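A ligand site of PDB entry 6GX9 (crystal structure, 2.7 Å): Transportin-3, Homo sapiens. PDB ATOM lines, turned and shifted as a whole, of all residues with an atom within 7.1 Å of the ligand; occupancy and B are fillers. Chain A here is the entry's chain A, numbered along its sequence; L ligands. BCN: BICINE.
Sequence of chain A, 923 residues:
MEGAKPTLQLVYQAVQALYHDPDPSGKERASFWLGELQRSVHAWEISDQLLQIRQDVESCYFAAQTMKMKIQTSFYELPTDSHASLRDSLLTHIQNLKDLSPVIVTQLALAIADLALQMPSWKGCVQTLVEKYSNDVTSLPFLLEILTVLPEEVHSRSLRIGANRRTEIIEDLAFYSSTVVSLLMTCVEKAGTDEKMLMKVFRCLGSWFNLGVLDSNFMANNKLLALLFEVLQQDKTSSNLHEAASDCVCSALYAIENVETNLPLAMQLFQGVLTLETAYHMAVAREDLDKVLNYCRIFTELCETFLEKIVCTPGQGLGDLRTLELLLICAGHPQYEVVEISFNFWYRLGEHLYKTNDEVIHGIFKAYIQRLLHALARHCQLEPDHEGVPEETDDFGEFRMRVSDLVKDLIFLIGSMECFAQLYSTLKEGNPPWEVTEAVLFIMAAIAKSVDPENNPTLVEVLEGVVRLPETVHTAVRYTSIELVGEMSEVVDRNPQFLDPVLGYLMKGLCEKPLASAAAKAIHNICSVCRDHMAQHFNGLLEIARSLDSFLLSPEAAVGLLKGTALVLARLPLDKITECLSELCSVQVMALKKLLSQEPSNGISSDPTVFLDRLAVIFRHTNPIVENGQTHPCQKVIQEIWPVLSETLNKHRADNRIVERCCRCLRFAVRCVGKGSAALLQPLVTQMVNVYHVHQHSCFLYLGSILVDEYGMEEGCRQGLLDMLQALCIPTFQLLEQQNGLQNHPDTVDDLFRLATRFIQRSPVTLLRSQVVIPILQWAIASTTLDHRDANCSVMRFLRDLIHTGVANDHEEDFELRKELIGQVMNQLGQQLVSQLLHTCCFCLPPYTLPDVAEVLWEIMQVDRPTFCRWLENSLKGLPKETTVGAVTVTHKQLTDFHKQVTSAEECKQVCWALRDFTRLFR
O of Ala 116 sits at hydrogen-bond distance from O4 of the ligand (2.8 Å). The backbone NH (N) of Val 126 lies within hydrogen-bond range of an oxygen (O6) of the ligand (3.3 Å). O of Trp 122 lies close to O4 of the ligand (3.5 Å). An oxygen (O4) of the ligand lies within hydrogen-bond range of the backbone carbonyl oxygen of Met 119, at 3.2 Å. The backbone NH of Cys 125 is in hydrogen-bond range of an oxygen (O6) of the ligand. OD2 of Asp 172 is in salt-bridge range of N1 of the ligand. The guanidinium group (NH2) of Arg 165 is in salt-bridge range of an oxygen (O22) of the ligand, 2.7 Å away.
OE1 of Glu 168 lies within salt-bridge range of NH1 of Arg 165 (3.3 Å). NE1 of Trp 122 lies within hydrogen-bond range of OG1 of Thr 128. The backbone carbonyl oxygen (O) of Cys 125 is in hydrogen-bond range of the side-chain hydroxyl (OG1) of Thr 128.
CA of Gly 124 touches O6 of the ligand, at 3.4 Å. Ile 169 touches the ligand (CD1 to C1, 3.6 Å). Leu 173 touches the ligand (CD2 to C5, 3.9 Å). CD2 of Tyr 176 touches O6 of the ligand, 3.4 Å away. Hydrophobic or aromatic side chains within 4 Å of the ligand: Ala 116, Val 126, Ile 169, Leu 173 and Tyr 176. 11 residues have an atom within 4 Å of the ligand: Ala 116, Met 119, Trp 122, Gly 124, Cys 125, Val 126, Arg 165, Ile 169, Asp 172, Leu 173 and Tyr 176. The nearest printed residue that does not touch the ligand is Glu 168 (4.1 Å).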
ATOM      1  N   ALA A 113       9.423  33.280  12.397  1.00  0.00           N
ATOM      2  CA  ALA A 113       8.466  32.233  12.733  1.00  0.00           C
ATOM      3  C   ALA A 113       8.906  30.889  12.168  1.00  0.00           C
ATOM      4  O   ALA A 113       8.947  29.881  12.886  1.00  0.00           O
ATOM      5  CB  ALA A 113       7.078  32.613  12.217  1.00  0.00           C
ATOM      6  N   LEU A 115      11.855  29.987  11.344  1.00  0.00           N
ATOM      7  CA  LEU A 115      13.068  29.548  12.016  1.00  0.00           C
ATOM      8  C   LEU A 115      12.746  28.879  13.349  1.00  0.00           C
ATOM      9  O   LEU A 115      13.301  27.820  13.665  1.00  0.00           O
ATOM     10  CB  LEU A 115      14.025  30.724  12.209  1.00  0.00           C
ATOM     11  CG  LEU A 115      15.294  30.438  13.001  1.00  0.00           C
ATOM     12  CD1 LEU A 115      16.056  29.285  12.379  1.00  0.00           C
ATOM     13  CD2 LEU A 115      16.174  31.671  13.057  1.00  0.00           C
ATOM     14  N   ALA A 116      11.853  29.480  14.133  1.00  0.00           N
ATOM     15  CA  ALA A 116      11.489  28.907  15.420  1.00  0.00           C
ATOM     16  C   ALA A 116      10.866  27.521  15.252  1.00  0.00           C
ATOM     17  O   ALA A 116      11.188  26.593  16.004  1.00  0.00           O
ATOM     18  CB  ALA A 116      10.541  29.845  16.169  1.00  0.00           C
ATOM     19  N   LEU A 117       9.980  27.360  14.262  1.00  0.00           N
ATOM     20  CA  LEU A 117       9.301  26.094  14.059  1.00  0.00           C
ATOM     21  C   LEU A 117      10.270  24.964  13.698  1.00  0.00           C
ATOM     22  O   LEU A 117       9.944  23.796  13.916  1.00  0.00           O
ATOM     23  CB  LEU A 117       8.238  26.228  12.969  1.00  0.00           C
ATOM     24  CG  LEU A 117       7.092  27.178  13.313  1.00  0.00           C
ATOM     25  CD1 LEU A 117       6.071  27.201  12.194  1.00  0.00           C
ATOM     26  CD2 LEU A 117       6.445  26.789  14.634  1.00  0.00           C
ATOM     27  N   GLN A 118      11.426  25.283  13.143  1.00  0.00           N
ATOM     28  CA  GLN A 118      12.415  24.287  12.764  1.00  0.00           C
ATOM     29  C   GLN A 118      13.596  24.237  13.724  1.00  0.00           C
ATOM     30  O   GLN A 118      14.558  23.500  13.467  1.00  0.00           O
ATOM     31  CB  GLN A 118      12.921  24.564  11.342  1.00  0.00           C
ATOM     32  CG  GLN A 118      11.843  24.546  10.281  1.00  0.00           C
ATOM     33  CD  GLN A 118      12.360  24.949   8.918  1.00  0.00           C
ATOM     34  OE1 GLN A 118      12.821  24.123   8.143  1.00  0.00           O
ATOM     35  NE2 GLN A 118      12.279  26.240   8.621  1.00  0.00           N
ATOM     36  N   MET A 119      13.561  24.991  14.821  1.00  0.00           N
ATOM     37  CA  MET A 119      14.649  25.055  15.790  1.00  0.00           C
ATOM     38  C   MET A 119      14.109  24.650  17.156  1.00  0.00           C
ATOM     39  O   MET A 119      13.668  25.508  17.933  1.00  0.00           O
ATOM     40  CB  MET A 119      15.273  26.447  15.821  1.00  0.00           C
ATOM     41  CG  MET A 119      16.456  26.579  16.769  1.00  0.00           C
ATOM     42  SD  MET A 119      17.346  28.143  16.559  1.00  0.00           S
ATOM     43  CE  MET A 119      15.979  29.280  16.374  1.00  0.00           C
ATOM     44  N   PRO A 120      14.082  23.348  17.475  1.00  0.00           N
ATOM     45  CA  PRO A 120      13.575  22.936  18.794  1.00  0.00           C
ATOM     46  C   PRO A 120      14.430  23.429  19.954  1.00  0.00           C
ATOM     47  O   PRO A 120      13.913  23.503  21.075  1.00  0.00           O
ATOM     48  CB  PRO A 120      13.591  21.400  18.707  1.00  0.00           C
ATOM     49  CG  PRO A 120      13.617  21.094  17.233  1.00  0.00           C
ATOM     50  CD  PRO A 120      14.413  22.201  16.613  1.00  0.00           C
ATOM     51  N   SER A 121      15.696  23.770  19.720  1.00  0.00           N
ATOM     52  CA  SER A 121      16.544  24.286  20.782  1.00  0.00           C
ATOM     53  C   SER A 121      16.068  25.637  21.286  1.00  0.00           C
ATOM     54  O   SER A 121      16.418  26.033  22.403  1.00  0.00           O
ATOM     55  CB  SER A 121      17.995  24.385  20.312  1.00  0.00           C
ATOM     56  OG  SER A 121      18.079  24.967  19.029  1.00  0.00           O
ATOM     57  N   TRP A 122      15.285  26.374  20.488  1.00  0.00           N
ATOM     58  CA  TRP A 122      14.692  27.630  20.924  1.00  0.00           C
ATOM     59  C   TRP A 122      13.419  27.324  21.713  1.00  0.00           C
ATOM     60  O   TRP A 122      12.283  27.504  21.251  1.00  0.00           O
ATOM     61  CB  TRP A 122      14.417  28.539  19.734  1.00  0.00           C
ATOM     62  CG  TRP A 122      14.053  29.960  20.119  1.00  0.00           C
ATOM     63  CD1 TRP A 122      14.076  30.485  21.371  1.00  0.00           C
ATOM     64  CD2 TRP A 122      13.626  31.002  19.244  1.00  0.00           C
ATOM     65  NE1 TRP A 122      13.682  31.808  21.330  1.00  0.00           N
ATOM     66  CE2 TRP A 122      13.405  32.149  20.033  1.00  0.00           C
ATOM     67  CE3 TRP A 122      13.414  31.082  17.858  1.00  0.00           C
ATOM     68  CZ2 TRP A 122      12.970  33.355  19.497  1.00  0.00           C
ATOM     69  CZ3 TRP A 122      12.990  32.285  17.323  1.00  0.00           C
ATOM     70  CH2 TRP A 122      12.770  33.411  18.137  1.00  0.00           C
ATOM     71  N   LYS A 123      13.615  26.828  22.930  1.00  0.00           N
ATOM     72  CA  LYS A 123      12.510  26.433  23.781  1.00  0.00           C
ATOM     73  C   LYS A 123      11.804  27.656  24.350  1.00  0.00           C
ATOM     74  O   LYS A 123      12.444  28.600  24.818  1.00  0.00           O
ATOM     75  CB  LYS A 123      13.006  25.549  24.916  1.00  0.00           C
ATOM     76  CG  LYS A 123      13.671  24.248  24.451  1.00  0.00           C
ATOM     77  CD  LYS A 123      14.113  23.406  25.638  1.00  0.00           C
ATOM     78  CE  LYS A 123      14.746  22.104  25.190  1.00  0.00           C
ATOM     79  NZ  LYS A 123      15.156  21.253  26.350  1.00  0.00           N
ATOM     80  N   GLY A 124      10.472  27.629  24.312  1.00  0.00           N
ATOM     81  CA  GLY A 124       9.674  28.734  24.813  1.00  0.00           C
ATOM     82  C   GLY A 124       9.951  30.039  24.077  1.00  0.00           C
ATOM     83  O   GLY A 124      10.146  31.073  24.709  1.00  0.00           O
ATOM     84  N   CYS A 125       9.946  29.982  22.744  1.00  0.00           N
ATOM     85  CA  CYS A 125      10.305  31.162  21.960  1.00  0.00           C
ATOM     86  C   CYS A 125       9.305  32.297  22.189  1.00  0.00           C
ATOM     87  O   CYS A 125       9.697  33.469  22.225  1.00  0.00           O
ATOM     88  CB  CYS A 125      10.371  30.810  20.475  1.00  0.00           C
ATOM     89  SG  CYS A 125       8.777  30.596  19.679  1.00  0.00           S
ATOM     90  N   VAL A 126       8.028  31.968  22.344  1.00  0.00           N
ATOM     91  CA  VAL A 126       7.019  33.006  22.590  1.00  0.00           C
ATOM     92  C   VAL A 126       7.330  33.741  23.885  1.00  0.00           C
ATOM     93  O   VAL A 126       7.246  34.971  23.952  1.00  0.00           O
ATOM     94  CB  VAL A 126       5.615  32.388  22.613  1.00  0.00           C
ATOM     95  CG1 VAL A 126       4.606  33.392  23.158  1.00  0.00           C
ATOM     96  CG2 VAL A 126       5.208  31.940  21.212  1.00  0.00           C
ATOM     97  N   GLN A 127       7.732  33.009  24.919  1.00  0.00           N
ATOM     98  CA  GLN A 127       8.052  33.632  26.203  1.00  0.00           C
ATOM     99  C   GLN A 127       9.268  34.543  26.070  1.00  0.00           C
ATOM    100  O   GLN A 127       9.239  35.697  26.529  1.00  0.00           O
ATOM    101  CB  GLN A 127       8.300  32.558  27.252  1.00  0.00           C
ATOM    102  CG  GLN A 127       8.944  33.069  28.534  1.00  0.00           C
ATOM    103  CD  GLN A 127       7.935  33.478  29.567  1.00  0.00           C
ATOM    104  OE1 GLN A 127       6.844  33.954  29.242  1.00  0.00           O
ATOM    105  NE2 GLN A 127       8.283  33.301  30.844  1.00  0.00           N
ATOM    106  N   THR A 128      10.333  34.065  25.437  1.00  0.00           N
ATOM    107  CA  THR A 128      11.531  34.874  25.277  1.00  0.00           C
ATOM    108  C   THR A 128      11.254  36.118  24.456  1.00  0.00           C
ATOM    109  O   THR A 128      11.811  37.194  24.727  1.00  0.00           O
ATOM    110  CB  THR A 128      12.653  34.053  24.634  1.00  0.00           C
ATOM    111  OG1 THR A 128      12.256  33.628  23.325  1.00  0.00           O
ATOM    112  CG2 THR A 128      12.964  32.825  25.477  1.00  0.00           C
ATOM    113  N   LEU A 150       3.180  33.329  13.435  1.00  0.00           N
ATOM    114  CA  LEU A 150       3.692  32.066  13.963  1.00  0.00           C
ATOM    115  C   LEU A 150       2.620  30.983  14.011  1.00  0.00           C
ATOM    116  O   LEU A 150       2.890  29.862  13.536  1.00  0.00           O
ATOM    117  CB  LEU A 150       4.316  32.285  15.343  1.00  0.00           C
ATOM    118  CG  LEU A 150       4.909  31.050  16.023  1.00  0.00           C
ATOM    119  CD1 LEU A 150       5.987  30.421  15.163  1.00  0.00           C
ATOM    120  CD2 LEU A 150       5.458  31.404  17.396  1.00  0.00           C
ATOM    121  N   ARG A 165       6.124  16.629  15.389  1.00  0.00           N
ATOM    122  CA  ARG A 165       6.679  17.931  15.728  1.00  0.00           C
ATOM    123  C   ARG A 165       5.583  18.988  15.815  1.00  0.00           C
ATOM    124  O   ARG A 165       5.585  19.824  16.721  1.00  0.00           O
ATOM    125  CB  ARG A 165       7.740  18.345  14.701  1.00  0.00           C
ATOM    126  CG  ARG A 165       8.306  19.728  14.926  1.00  0.00           C
ATOM    127  CD  ARG A 165       9.410  19.721  15.964  1.00  0.00           C
ATOM    128  NE  ARG A 165       9.922  21.068  16.219  1.00  0.00           N
ATOM    129  CZ  ARG A 165       9.772  21.725  17.357  1.00  0.00           C
ATOM    130  NH1 ARG A 165       9.137  21.157  18.373  1.00  0.00           N
ATOM    131  NH2 ARG A 165      10.268  22.952  17.488  1.00  0.00           N
ATOM    132  N   GLU A 168       3.949  18.803  19.082  1.00  0.00           N
ATOM    133  CA  GLU A 168       4.793  19.436  20.092  1.00  0.00           C
ATOM    134  C   GLU A 168       4.656  20.953  20.037  1.00  0.00           C
ATOM    135  O   GLU A 168       4.512  21.605  21.081  1.00  0.00           O
ATOM    136  CB  GLU A 168       6.247  19.037  19.889  1.00  0.00           C
ATOM    137  CG  GLU A 168       6.595  17.617  20.312  1.00  0.00           C
ATOM    138  CD  GLU A 168       8.039  17.270  20.016  1.00  0.00           C
ATOM    139  OE1 GLU A 168       8.850  18.201  19.787  1.00  0.00           O
ATOM    140  OE2 GLU A 168       8.375  16.057  20.003  1.00  0.00           O
ATOM    141  N   ILE A 169       4.678  21.521  18.831  1.00  0.00           N
ATOM    142  CA  ILE A 169       4.571  22.974  18.682  1.00  0.00           C
ATOM    143  C   ILE A 169       3.244  23.465  19.242  1.00  0.00           C
ATOM    144  O   ILE A 169       3.193  24.441  20.014  1.00  0.00           O
ATOM    145  CB  ILE A 169       4.730  23.373  17.209  1.00  0.00           C
ATOM    146  CG1 ILE A 169       6.105  22.978  16.665  1.00  0.00           C
ATOM    147  CG2 ILE A 169       4.481  24.871  17.036  1.00  0.00           C
ATOM    148  CD1 ILE A 169       7.186  23.990  16.938  1.00  0.00           C
ATOM    149  N   ILE A 170       2.148  22.807  18.869  1.00  0.00           N
ATOM    150  CA  ILE A 170       0.817  23.299  19.212  1.00  0.00           C
ATOM    151  C   ILE A 170       0.601  23.252  20.725  1.00  0.00           C
ATOM    152  O   ILE A 170       0.059  24.184  21.320  1.00  0.00           O
ATOM    153  CB  ILE A 170      -0.267  22.517  18.450  1.00  0.00           C
ATOM    154  CG1 ILE A 170      -0.197  22.855  16.956  1.00  0.00           C
ATOM    155  CG2 ILE A 170      -1.637  22.853  18.985  1.00  0.00           C
ATOM    156  CD1 ILE A 170      -1.185  22.094  16.109  1.00  0.00           C
ATOM    157  N   GLU A 171       1.031  22.166  21.375  1.00  0.00           N
ATOM    158  CA  GLU A 171       0.874  22.088  22.817  1.00  0.00           C
ATOM    159  C   GLU A 171       1.880  22.957  23.555  1.00  0.00           C
ATOM    160  O   GLU A 171       1.662  23.281  24.728  1.00  0.00           O
ATOM    161  CB  GLU A 171       0.970  20.643  23.299  1.00  0.00           C
ATOM    162  CG  GLU A 171       2.363  20.039  23.262  1.00  0.00           C
ATOM    163  CD  GLU A 171       2.377  18.600  23.750  1.00  0.00           C
ATOM    164  OE1 GLU A 171       1.449  17.844  23.410  1.00  0.00           O
ATOM    165  OE2 GLU A 171       3.327  18.238  24.475  1.00  0.00           O
ATOM    166  N   ASP A 172       2.965  23.363  22.892  1.00  0.00           N
ATOM    167  CA  ASP A 172       3.882  24.327  23.506  1.00  0.00           C
ATOM    168  C   ASP A 172       3.359  25.749  23.344  1.00  0.00           C
ATOM    169  O   ASP A 172       3.515  26.572  24.251  1.00  0.00           O
ATOM    170  CB  ASP A 172       5.275  24.190  22.885  1.00  0.00           C
ATOM    171  CG  ASP A 172       6.371  24.469  23.893  1.00  0.00           C
ATOM    172  OD1 ASP A 172       6.092  24.487  25.105  1.00  0.00           O
ATOM    173  OD2 ASP A 172       7.527  24.672  23.462  1.00  0.00           O
ATOM    174  N   LEU A 173       2.736  26.055  22.207  1.00  0.00           N
ATOM    175  CA  LEU A 173       2.117  27.358  22.027  1.00  0.00           C
ATOM    176  C   LEU A 173       0.910  27.524  22.942  1.00  0.00           C
ATOM    177  O   LEU A 173       0.653  28.627  23.451  1.00  0.00           O
ATOM    178  CB  LEU A 173       1.717  27.564  20.568  1.00  0.00           C
ATOM    179  CG  LEU A 173       2.857  27.678  19.549  1.00  0.00           C
ATOM    180  CD1 LEU A 173       2.312  27.684  18.131  1.00  0.00           C
ATOM    181  CD2 LEU A 173       3.672  28.919  19.801  1.00  0.00           C
ATOM    182  N   TYR A 176       1.824  28.683  26.461  1.00  0.00           N
ATOM    183  CA  TYR A 176       2.125  30.100  26.587  1.00  0.00           C
ATOM    184  C   TYR A 176       1.002  30.996  26.085  1.00  0.00           C
ATOM    185  O   TYR A 176       1.201  32.204  25.916  1.00  0.00           O
ATOM    186  CB  TYR A 176       3.426  30.440  25.844  1.00  0.00           C
ATOM    187  CG  TYR A 176       4.650  29.813  26.469  1.00  0.00           C
ATOM    188  CD1 TYR A 176       5.224  30.342  27.616  1.00  0.00           C
ATOM    189  CD2 TYR A 176       5.237  28.683  25.902  1.00  0.00           C
ATOM    190  CE1 TYR A 176       6.341  29.763  28.186  1.00  0.00           C
ATOM    191  CE2 TYR A 176       6.352  28.098  26.464  1.00  0.00           C
ATOM    192  CZ  TYR A 176       6.901  28.644  27.603  1.00  0.00           C
ATOM    193  OH  TYR A 176       8.020  28.072  28.168  1.00  0.00           O
ATOM    194  N   TRP A 208      -4.597  33.235  16.978  1.00  0.00           N
ATOM    195  CA  TRP A 208      -4.488  32.268  18.059  1.00  0.00           C
ATOM    196  C   TRP A 208      -5.798  31.521  18.288  1.00  0.00           C
ATOM    197  O   TRP A 208      -5.789  30.384  18.770  1.00  0.00           O
ATOM    198  CB  TRP A 208      -4.002  32.952  19.330  1.00  0.00           C
ATOM    199  CG  TRP A 208      -2.521  33.190  19.307  1.00  0.00           C
ATOM    200  CD1 TRP A 208      -1.858  34.133  18.570  1.00  0.00           C
ATOM    201  CD2 TRP A 208      -1.517  32.476  20.028  1.00  0.00           C
ATOM    202  NE1 TRP A 208      -0.511  34.042  18.791  1.00  0.00           N
ATOM    203  CE2 TRP A 208      -0.273  33.040  19.686  1.00  0.00           C
ATOM    204  CE3 TRP A 208      -1.557  31.419  20.944  1.00  0.00           C
ATOM    205  CZ2 TRP A 208       0.930  32.572  20.221  1.00  0.00           C
ATOM    206  CZ3 TRP A 208      -0.361  30.962  21.473  1.00  0.00           C
ATOM    207  CH2 TRP A 208       0.866  31.534  21.116  1.00  0.00           C
HETATM  208  N1  BCN L   1       8.122  26.651  20.296  1.00  0.00           N
HETATM  209  C1  BCN L   1       7.564  25.300  20.229  1.00  0.00           C
HETATM  210  C2  BCN L   1       8.613  24.236  20.489  1.00  0.00           C
HETATM  211  O21 BCN L   1       8.250  23.222  21.128  1.00  0.00           O
HETATM  212  O22 BCN L   1       9.634  24.231  19.767  1.00  0.00           O
HETATM  213  C3  BCN L   1       8.480  27.119  18.946  1.00  0.00           C
HETATM  214  C4  BCN L   1      10.002  27.231  18.856  1.00  0.00           C
HETATM  215  O4  BCN L   1      10.574  25.923  18.660  1.00  0.00           O
HETATM  216  C5  BCN L   1       7.131  27.579  20.865  1.00  0.00           C
HETATM  217  C6  BCN L   1       7.305  27.649  22.373  1.00  0.00           C
HETATM  218  O6  BCN L   1       6.845  28.909  22.863  1.00  0.00           O
